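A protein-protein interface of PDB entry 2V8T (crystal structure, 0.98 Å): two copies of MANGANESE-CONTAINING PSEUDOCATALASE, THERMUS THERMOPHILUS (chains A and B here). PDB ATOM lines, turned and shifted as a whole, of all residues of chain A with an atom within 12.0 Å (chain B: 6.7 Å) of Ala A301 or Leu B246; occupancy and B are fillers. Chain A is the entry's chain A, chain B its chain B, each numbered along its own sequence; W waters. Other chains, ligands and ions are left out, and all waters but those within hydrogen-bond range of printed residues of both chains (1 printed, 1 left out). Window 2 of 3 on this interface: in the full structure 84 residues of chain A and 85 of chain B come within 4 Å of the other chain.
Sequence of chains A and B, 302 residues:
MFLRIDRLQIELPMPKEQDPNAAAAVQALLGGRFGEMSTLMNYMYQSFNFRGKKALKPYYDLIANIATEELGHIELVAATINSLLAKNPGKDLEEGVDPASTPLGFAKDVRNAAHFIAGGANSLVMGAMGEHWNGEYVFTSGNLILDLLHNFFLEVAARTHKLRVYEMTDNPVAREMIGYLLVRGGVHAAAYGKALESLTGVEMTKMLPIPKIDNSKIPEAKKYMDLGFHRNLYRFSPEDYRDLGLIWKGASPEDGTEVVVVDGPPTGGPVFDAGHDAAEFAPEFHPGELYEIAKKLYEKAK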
ATOM      1  N   LEU A 290     -29.450   3.823   2.765  1.00  0.00           N
ATOM      2  CA  LEU A 290     -29.202   3.057   3.994  1.00  0.00           C
ATOM      3  C   LEU A 290     -28.338   1.837   3.691  1.00  0.00           C
ATOM      4  O   LEU A 290     -27.461   1.477   4.497  1.00  0.00           O
ATOM      5  CB  LEU A 290     -30.508   2.601   4.673  1.00  0.00           C
ATOM      6  CG  LEU A 290     -31.431   3.747   5.109  1.00  0.00           C
ATOM      7  CD1 LEU A 290     -32.526   3.176   6.034  1.00  0.00           C
ATOM      8  CD2 LEU A 290     -30.691   4.921   5.769  1.00  0.00           C
ATOM      9  N   TYR A 291     -28.537   1.208   2.543  1.00  0.00           N
ATOM     10  CA  TYR A 291     -27.684   0.073   2.154  1.00  0.00           C
ATOM     11  C   TYR A 291     -26.224   0.531   2.041  1.00  0.00           C
ATOM     12  O   TYR A 291     -25.312  -0.216   2.395  1.00  0.00           O
ATOM     13  CB  TYR A 291     -28.147  -0.569   0.874  1.00  0.00           C
ATOM     14  CG  TYR A 291     -29.522  -1.202   0.893  1.00  0.00           C
ATOM     15  CD1 TYR A 291     -30.178  -1.558   2.066  1.00  0.00           C
ATOM     16  CD2 TYR A 291     -30.168  -1.447  -0.305  1.00  0.00           C
ATOM     17  CE1 TYR A 291     -31.420  -2.144   2.049  1.00  0.00           C
ATOM     18  CE2 TYR A 291     -31.421  -2.060  -0.346  1.00  0.00           C
ATOM     19  CZ  TYR A 291     -32.048  -2.414   0.848  1.00  0.00           C
ATOM     20  OH  TYR A 291     -33.290  -2.992   0.843  1.00  0.00           O
ATOM     21  N   GLU A 292     -26.012   1.736   1.511  1.00  0.00           N
ATOM     22  CA  GLU A 292     -24.656   2.276   1.423  1.00  0.00           C
ATOM     23  C   GLU A 292     -24.056   2.537   2.773  1.00  0.00           C
ATOM     24  O   GLU A 292     -22.870   2.302   3.012  1.00  0.00           O
ATOM     25  CB  GLU A 292     -24.658   3.493   0.506  1.00  0.00           C
ATOM     26  CG  GLU A 292     -23.331   4.129   0.294  1.00  0.00           C
ATOM     27  CD  GLU A 292     -22.299   3.272  -0.396  1.00  0.00           C
ATOM     28  OE1 GLU A 292     -22.603   2.229  -1.002  1.00  0.00           O
ATOM     29  OE2 GLU A 292     -21.120   3.704  -0.346  1.00  0.00           O
ATOM     30  N   ILE A 293     -24.847   3.070   3.714  1.00  0.00           N
ATOM     31  CA  ILE A 293     -24.386   3.283   5.090  1.00  0.00           C
ATOM     32  C   ILE A 293     -23.915   1.944   5.660  1.00  0.00           C
ATOM     33  O   ILE A 293     -22.851   1.858   6.294  1.00  0.00           O
ATOM     34  CB  ILE A 293     -25.464   3.953   5.964  1.00  0.00           C
ATOM     35  CG1 ILE A 293     -25.651   5.394   5.516  1.00  0.00           C
ATOM     36  CG2 ILE A 293     -25.173   3.837   7.434  1.00  0.00           C
ATOM     37  CD1 ILE A 293     -26.841   6.081   6.171  1.00  0.00           C
ATOM     38  N   ALA A 294     -24.733   0.894   5.494  1.00  0.00           N
ATOM     39  CA  ALA A 294     -24.368  -0.412   6.050  1.00  0.00           C
ATOM     40  C   ALA A 294     -23.073  -0.918   5.426  1.00  0.00           C
ATOM     41  O   ALA A 294     -22.199  -1.420   6.130  1.00  0.00           O
ATOM     42  CB  ALA A 294     -25.497  -1.394   5.841  1.00  0.00           C
ATOM     43  N   LYS A 295     -22.950  -0.779   4.109  1.00  0.00           N
ATOM     44  CA  LYS A 295     -21.703  -1.205   3.430  1.00  0.00           C
ATOM     45  C   LYS A 295     -20.501  -0.493   4.042  1.00  0.00           C
ATOM     46  O   LYS A 295     -19.421  -1.086   4.258  1.00  0.00           O
ATOM     47  CB  LYS A 295     -21.729  -0.847   1.945  1.00  0.00           C
ATOM     48  CG  LYS A 295     -22.534  -1.777   1.149  1.00  0.00           C
ATOM     49  CD  LYS A 295     -22.626  -1.310  -0.266  1.00  0.00           C
ATOM     50  CE  LYS A 295     -23.485  -2.216  -1.107  1.00  0.00           C
ATOM     51  NZ  LYS A 295     -23.699  -1.665  -2.505  1.00  0.00           N
ATOM     52  N   LYS A 296     -20.622   0.801   4.266  1.00  0.00           N
ATOM     53  CA  LYS A 296     -19.497   1.555   4.801  1.00  0.00           C
ATOM     54  C   LYS A 296     -19.146   1.166   6.242  1.00  0.00           C
ATOM     55  O   LYS A 296     -17.975   1.253   6.626  1.00  0.00           O
ATOM     56  CB  LYS A 296     -19.768   3.065   4.679  1.00  0.00           C
ATOM     57  CG  LYS A 296     -19.710   3.580   3.242  1.00  0.00           C
ATOM     58  CD  LYS A 296     -18.751   2.823   2.281  1.00  0.00           C
ATOM     59  CE  LYS A 296     -18.602   3.541   0.950  1.00  0.00           C
ATOM     60  NZ  LYS A 296     -18.274   4.949   1.212  1.00  0.00           N
ATOM     61  N   LEU A 297     -20.102   0.644   7.007  1.00  0.00           N
ATOM     62  CA  LEU A 297     -19.794   0.190   8.370  1.00  0.00           C
ATOM     63  C   LEU A 297     -18.742  -0.907   8.345  1.00  0.00           C
ATOM     64  O   LEU A 297     -17.902  -1.033   9.231  1.00  0.00           O
ATOM     65  CB  LEU A 297     -21.018  -0.376   9.094  1.00  0.00           C
ATOM     66  CG  LEU A 297     -22.084   0.650   9.498  1.00  0.00           C
ATOM     67  CD1 LEU A 297     -23.255  -0.114  10.102  1.00  0.00           C
ATOM     68  CD2 LEU A 297     -21.512   1.747  10.450  1.00  0.00           C
ATOM     69  N   TYR A 298     -18.803  -1.767   7.311  1.00  0.00           N
ATOM     70  CA  TYR A 298     -17.872  -2.885   7.172  1.00  0.00           C
ATOM     71  C   TYR A 298     -16.516  -2.356   6.769  1.00  0.00           C
ATOM     72  O   TYR A 298     -15.517  -2.985   7.070  1.00  0.00           O
ATOM     73  CB  TYR A 298     -18.363  -3.902   6.114  1.00  0.00           C
ATOM     74  CG  TYR A 298     -19.543  -4.769   6.601  1.00  0.00           C
ATOM     75  CD1 TYR A 298     -20.864  -4.378   6.453  1.00  0.00           C
ATOM     76  CD2 TYR A 298     -19.337  -5.933   7.288  1.00  0.00           C
ATOM     77  CE1 TYR A 298     -21.911  -5.124   6.936  1.00  0.00           C
ATOM     78  CE2 TYR A 298     -20.369  -6.710   7.779  1.00  0.00           C
ATOM     79  CZ  TYR A 298     -21.672  -6.300   7.621  1.00  0.00           C
ATOM     80  OH  TYR A 298     -22.747  -6.992   8.117  1.00  0.00           O
ATOM     81  N   GLU A 299     -16.462  -1.291   5.996  1.00  0.00           N
ATOM     82  CA  GLU A 299     -15.174  -0.720   5.545  1.00  0.00           C
ATOM     83  C   GLU A 299     -14.512  -0.176   6.743  1.00  0.00           C
ATOM     84  O   GLU A 299     -13.249  -0.223   6.799  1.00  0.00           O
ATOM     85  CB  GLU A 299     -15.455   0.357   4.536  1.00  0.00           C
ATOM     86  CG  GLU A 299     -15.960  -0.154   3.195  1.00  0.00           C
ATOM     87  CD  GLU A 299     -16.360   1.004   2.243  1.00  0.00           C
ATOM     88  OE1 GLU A 299     -16.009   2.178   2.518  1.00  0.00           O
ATOM     89  OE2 GLU A 299     -17.017   0.731   1.215  1.00  0.00           O
ATOM     90  N   LYS A 300     -15.221   0.389   7.694  1.00  0.00           N
ATOM     91  CA  LYS A 300     -14.603   0.937   8.882  1.00  0.00           C
ATOM     92  C   LYS A 300     -14.434  -0.109  10.037  1.00  0.00           C
ATOM     93  O   LYS A 300     -14.046   0.253  11.151  1.00  0.00           O
ATOM     94  CB  LYS A 300     -15.405   2.184   9.303  1.00  0.00           C
ATOM     95  CG  LYS A 300     -15.098   3.447   8.418  1.00  0.00           C
ATOM     96  CD  LYS A 300     -15.792   3.523   7.024  1.00  0.00           C
ATOM     97  CE  LYS A 300     -16.936   4.545   6.974  1.00  0.00           C
ATOM     98  NZ  LYS A 300     -17.072   5.257   5.679  1.00  0.00           N
ATOM     99  N   ALA A 301     -14.717  -1.388   9.763  1.00  0.00           N
ATOM    100  CA  ALA A 301     -14.575  -2.491  10.738  1.00  0.00           C
ATOM    101  C   ALA A 301     -13.128  -2.666  11.267  1.00  0.00           C
ATOM    102  O   ALA A 301     -12.153  -2.387  10.553  1.00  0.00           O
ATOM    103  CB  ALA A 301     -15.041  -3.810  10.111  1.00  0.00           C
ATOM    104  N   LYS A 302     -13.024  -3.176  12.499  1.00  0.00           N
ATOM    105  CA  LYS A 302     -11.747  -3.395  13.174  1.00  0.00           C
ATOM    106  C   LYS A 302     -11.158  -4.755  12.864  1.00  0.00           C
ATOM    107  O   LYS A 302     -10.057  -5.056  13.334  1.00  0.00           O
ATOM    108  CB  LYS A 302     -11.911  -3.254  14.695  1.00  0.00           C
ATOM    109  CG  LYS A 302     -12.322  -1.877  15.159  1.00  0.00           C
ATOM    110  CD  LYS A 302     -11.350  -0.801  14.689  1.00  0.00           C
ATOM    111  CE  LYS A 302     -11.761   0.566  15.177  1.00  0.00           C
ATOM    112  NZ  LYS A 302     -11.056   1.618  14.402  1.00  0.00           N
ATOM    113  N   PRO B  58     -25.944  -5.376   9.917  1.00  0.00           N
ATOM    114  CA  PRO B  58     -25.549  -5.034  11.309  1.00  0.00           C
ATOM    115  C   PRO B  58     -26.777  -4.690  12.167  1.00  0.00           C
ATOM    116  O   PRO B  58     -26.804  -4.976  13.371  1.00  0.00           O
ATOM    117  CB  PRO B  58     -24.595  -3.864  11.111  1.00  0.00           C
ATOM    118  CG  PRO B  58     -24.052  -4.090   9.653  1.00  0.00           C
ATOM    119  CD  PRO B  58     -25.222  -4.583   8.913  1.00  0.00           C
ATOM    120  N   SER B 198     -25.863   6.244  13.426  1.00  0.00           N
ATOM    121  CA  SER B 198     -25.245   5.737  12.227  1.00  0.00           C
ATOM    122  C   SER B 198     -26.136   5.941  10.993  1.00  0.00           C
ATOM    123  O   SER B 198     -25.619   6.123   9.893  1.00  0.00           O
ATOM    124  CB  SER B 198     -24.852   4.263  12.401  1.00  0.00           C
ATOM    125  OG  SER B 198     -25.912   3.370  12.370  1.00  0.00           O
ATOM    126  N   ARG B 242     -22.709 -11.946  14.039  1.00  0.00           N
ATOM    127  CA  ARG B 242     -21.312 -11.642  14.332  1.00  0.00           C
ATOM    128  C   ARG B 242     -20.873 -10.223  14.018  1.00  0.00           C
ATOM    129  O   ARG B 242     -19.714  -9.904  14.246  1.00  0.00           O
ATOM    130  CB  ARG B 242     -20.407 -12.585  13.494  1.00  0.00           C
ATOM    131  CG  ARG B 242     -20.532 -14.085  13.838  1.00  0.00           C
ATOM    132  CD  ARG B 242     -19.251 -14.953  13.602  1.00  0.00           C
ATOM    133  NE  ARG B 242     -19.265 -16.171  14.454  1.00  0.00           N
ATOM    134  CZ  ARG B 242     -18.289 -17.075  14.605  1.00  0.00           C
ATOM    135  NH1 ARG B 242     -17.154 -16.982  13.906  1.00  0.00           N
ATOM    136  NH2 ARG B 242     -18.452 -18.092  15.469  1.00  0.00           N
ATOM    137  N   ASP B 243     -21.795  -9.353  13.543  1.00  0.00           N
ATOM    138  CA  ASP B 243     -21.431  -8.005  13.137  1.00  0.00           C
ATOM    139  C   ASP B 243     -21.947  -6.935  14.117  1.00  0.00           C
ATOM    140  O   ASP B 243     -22.017  -5.759  13.753  1.00  0.00           O
ATOM    141  CB  ASP B 243     -21.902  -7.752  11.724  1.00  0.00           C
ATOM    142  CG  ASP B 243     -21.240  -8.673  10.722  1.00  0.00           C
ATOM    143  OD1 ASP B 243     -20.066  -9.029  10.896  1.00  0.00           O
ATOM    144  OD2 ASP B 243     -21.941  -9.036   9.710  1.00  0.00           O
ATOM    145  N   LEU B 244     -22.201  -7.313  15.375  1.00  0.00           N
ATOM    146  CA  LEU B 244     -22.684  -6.348  16.344  1.00  0.00           C
ATOM    147  C   LEU B 244     -21.729  -5.198  16.569  1.00  0.00           C
ATOM    148  O   LEU B 244     -22.156  -4.069  16.853  1.00  0.00           O
ATOM    149  CB  LEU B 244     -22.984  -7.047  17.656  1.00  0.00           C
ATOM    150  CG  LEU B 244     -24.114  -8.056  17.662  1.00  0.00           C
ATOM    151  CD1 LEU B 244     -24.092  -8.880  18.928  1.00  0.00           C
ATOM    152  CD2 LEU B 244     -25.459  -7.378  17.488  1.00  0.00           C
ATOM    153  N   GLY B 245     -20.425  -5.475  16.498  1.00  0.00           N
ATOM    154  CA  GLY B 245     -19.424  -4.460  16.804  1.00  0.00           C
ATOM    155  C   GLY B 245     -19.339  -3.355  15.784  1.00  0.00           C
ATOM    156  O   GLY B 245     -18.647  -2.357  16.029  1.00  0.00           O
ATOM    157  N   LEU B 246     -20.036  -3.478  14.647  1.00  0.00           N
ATOM    158  CA  LEU B 246     -20.083  -2.396  13.696  1.00  0.00           C
ATOM    159  C   LEU B 246     -20.901  -1.222  14.209  1.00  0.00           C
ATOM    160  O   LEU B 246     -20.746  -0.104  13.729  1.00  0.00           O
ATOM    161  CB  LEU B 246     -20.589  -2.855  12.359  1.00  0.00           C
ATOM    162  CG  LEU B 246     -19.685  -3.912  11.695  1.00  0.00           C
ATOM    163  CD1 LEU B 246     -20.271  -4.302  10.327  1.00  0.00           C
ATOM    164  CD2 LEU B 246     -18.203  -3.530  11.595  1.00  0.00           C
ATOM    165  N   ILE B 247     -21.847  -1.500  15.126  1.00  0.00           N
ATOM    166  CA  ILE B 247     -22.677  -0.524  15.783  1.00  0.00           C
ATOM    167  C   ILE B 247     -22.267  -0.339  17.230  1.00  0.00           C
ATOM    168  O   ILE B 247     -22.173   0.792  17.749  1.00  0.00           O
ATOM    169  CB  ILE B 247     -24.188  -0.878  15.674  1.00  0.00           C
ATOM    170  CG1 ILE B 247     -24.650  -0.930  14.242  1.00  0.00           C
ATOM    171  CG2 ILE B 247     -25.038   0.086  16.510  1.00  0.00           C
ATOM    172  CD1 ILE B 247     -25.978  -1.592  14.023  1.00  0.00           C
ATOM    173  N   TRP B 248     -22.064  -1.458  17.956  1.00  0.00           N
ATOM    174  CA  TRP B 248     -21.712  -1.443  19.363  1.00  0.00           C
ATOM    175  C   TRP B 248     -20.194  -1.255  19.481  1.00  0.00           C
ATOM    176  O   TRP B 248     -19.425  -2.212  19.524  1.00  0.00           O
ATOM    177  CB  TRP B 248     -22.166  -2.700  20.081  1.00  0.00           C
ATOM    178  CG  TRP B 248     -21.979  -2.615  21.540  1.00  0.00           C
ATOM    179  CD1 TRP B 248     -21.102  -3.346  22.318  1.00  0.00           C
ATOM    180  CD2 TRP B 248     -22.653  -1.731  22.456  1.00  0.00           C
ATOM    181  NE1 TRP B 248     -21.205  -2.980  23.635  1.00  0.00           N
ATOM    182  CE2 TRP B 248     -22.127  -1.966  23.759  1.00  0.00           C
ATOM    183  CE3 TRP B 248     -23.608  -0.707  22.297  1.00  0.00           C
ATOM    184  CZ2 TRP B 248     -22.531  -1.238  24.860  1.00  0.00           C
ATOM    185  CZ3 TRP B 248     -23.960   0.027  23.382  1.00  0.00           C
ATOM    186  CH2 TRP B 248     -23.438  -0.233  24.659  1.00  0.00           C
ATOM    187  N   LYS B 249     -19.806   0.001  19.457  1.00  0.00           N
ATOM    188  CA  LYS B 249     -18.415   0.462  19.509  1.00  0.00           C
ATOM    189  C   LYS B 249     -18.459   1.883  20.002  1.00  0.00           C
ATOM    190  O   LYS B 249     -19.511   2.529  20.069  1.00  0.00           O
ATOM    191  CB  LYS B 249     -17.744   0.358  18.119  1.00  0.00           C
ATOM    192  CG  LYS B 249     -18.384   1.215  17.009  1.00  0.00           C
ATOM    193  CD  LYS B 249     -17.667   1.123  15.649  1.00  0.00           C
ATOM    194  CE  LYS B 249     -18.209   2.119  14.601  1.00  0.00           C
ATOM    195  NZ  LYS B 249     -17.365   2.390  13.413  1.00  0.00           N
ATOM    196  N   VAL B 261     -18.250  -5.968  22.376  1.00  0.00           N
ATOM    197  CA  VAL B 261     -19.078  -7.135  22.191  1.00  0.00           C
ATOM    198  C   VAL B 261     -18.425  -8.316  22.924  1.00  0.00           C
ATOM    199  O   VAL B 261     -17.212  -8.520  22.816  1.00  0.00           O
ATOM    200  CB  VAL B 261     -19.268  -7.466  20.693  1.00  0.00           C
ATOM    201  CG1 VAL B 261     -20.083  -8.737  20.479  1.00  0.00           C
ATOM    202  CG2 VAL B 261     -19.942  -6.258  19.974  1.00  0.00           C
HETATM  203  O   HOH W   1     -18.359   0.306  12.017  1.00  0.00           O
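No position is printed for both chains.
Of the 6 pairs that touch across the chains among the printed residues, none has its exchanged pair printed and touching as well.
Ile A293 touches Ser B198.
Leu B246 touches Leu A297.
Pro B58 touches Tyr A298.
CE2 of Tyr A298 touches CD1 of Leu B246, 3.5 Å away.
CD2 of Leu B246 touches CB of Ala A301, at 3.5 Å.
Of chain A, only Leu A297 (3.5 Å), Tyr A298 (3.5 Å) and Ala A301 (3.5 Å) come within 4 Å of Leu B246.
Pro B58 touches one residue of chain A.
Of chain A, only Tyr A298 (2.7 Å) comes within 4 Å of Asp B243.
No residue of chain A comes within 4 Å of Ile B247.
Of the printed residues of chain A, Ser B198 touches Ile A293 (3.4 Å).
Of the printed residues of chain B, Ile A293 touches Ser B198.
Printed residues of chain B within 4 Å of Tyr A298: Pro B58 (3.5 Å), Asp B243 (2.7 Å) and Leu B246 (3.5 Å).
Lys A300 touches none of the printed residues of chain B.
Glu A292 touches none of the printed residues of chain B.
Water W1 lies within hydrogen-bond range of the side-chain amino group (NZ) of Lys B249, the backbone carbonyl oxygen (O) of Leu B246 and the backbone carbonyl oxygen (O) of Leu A297.
The side-chain hydroxyl of Tyr A298 sits at hydrogen-bond distance from the side-chain carboxylate of Asp B243, 2.7 Å away.
Of the 13 printed residues of chain A, 4 touch a printed residue of chain B.
Along chain A the printed residues that touch a printed residue of chain B span positions 293 to 301.
Printed residues of chain B that touch a printed residue of chain A: Pro B58, Ser B198, Asp B243 and Leu B246.
Along chain B the printed residues that touch a printed residue of chain A span positions 58 to 246.
Among the printed residues, 6 pairs touch across the chains.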
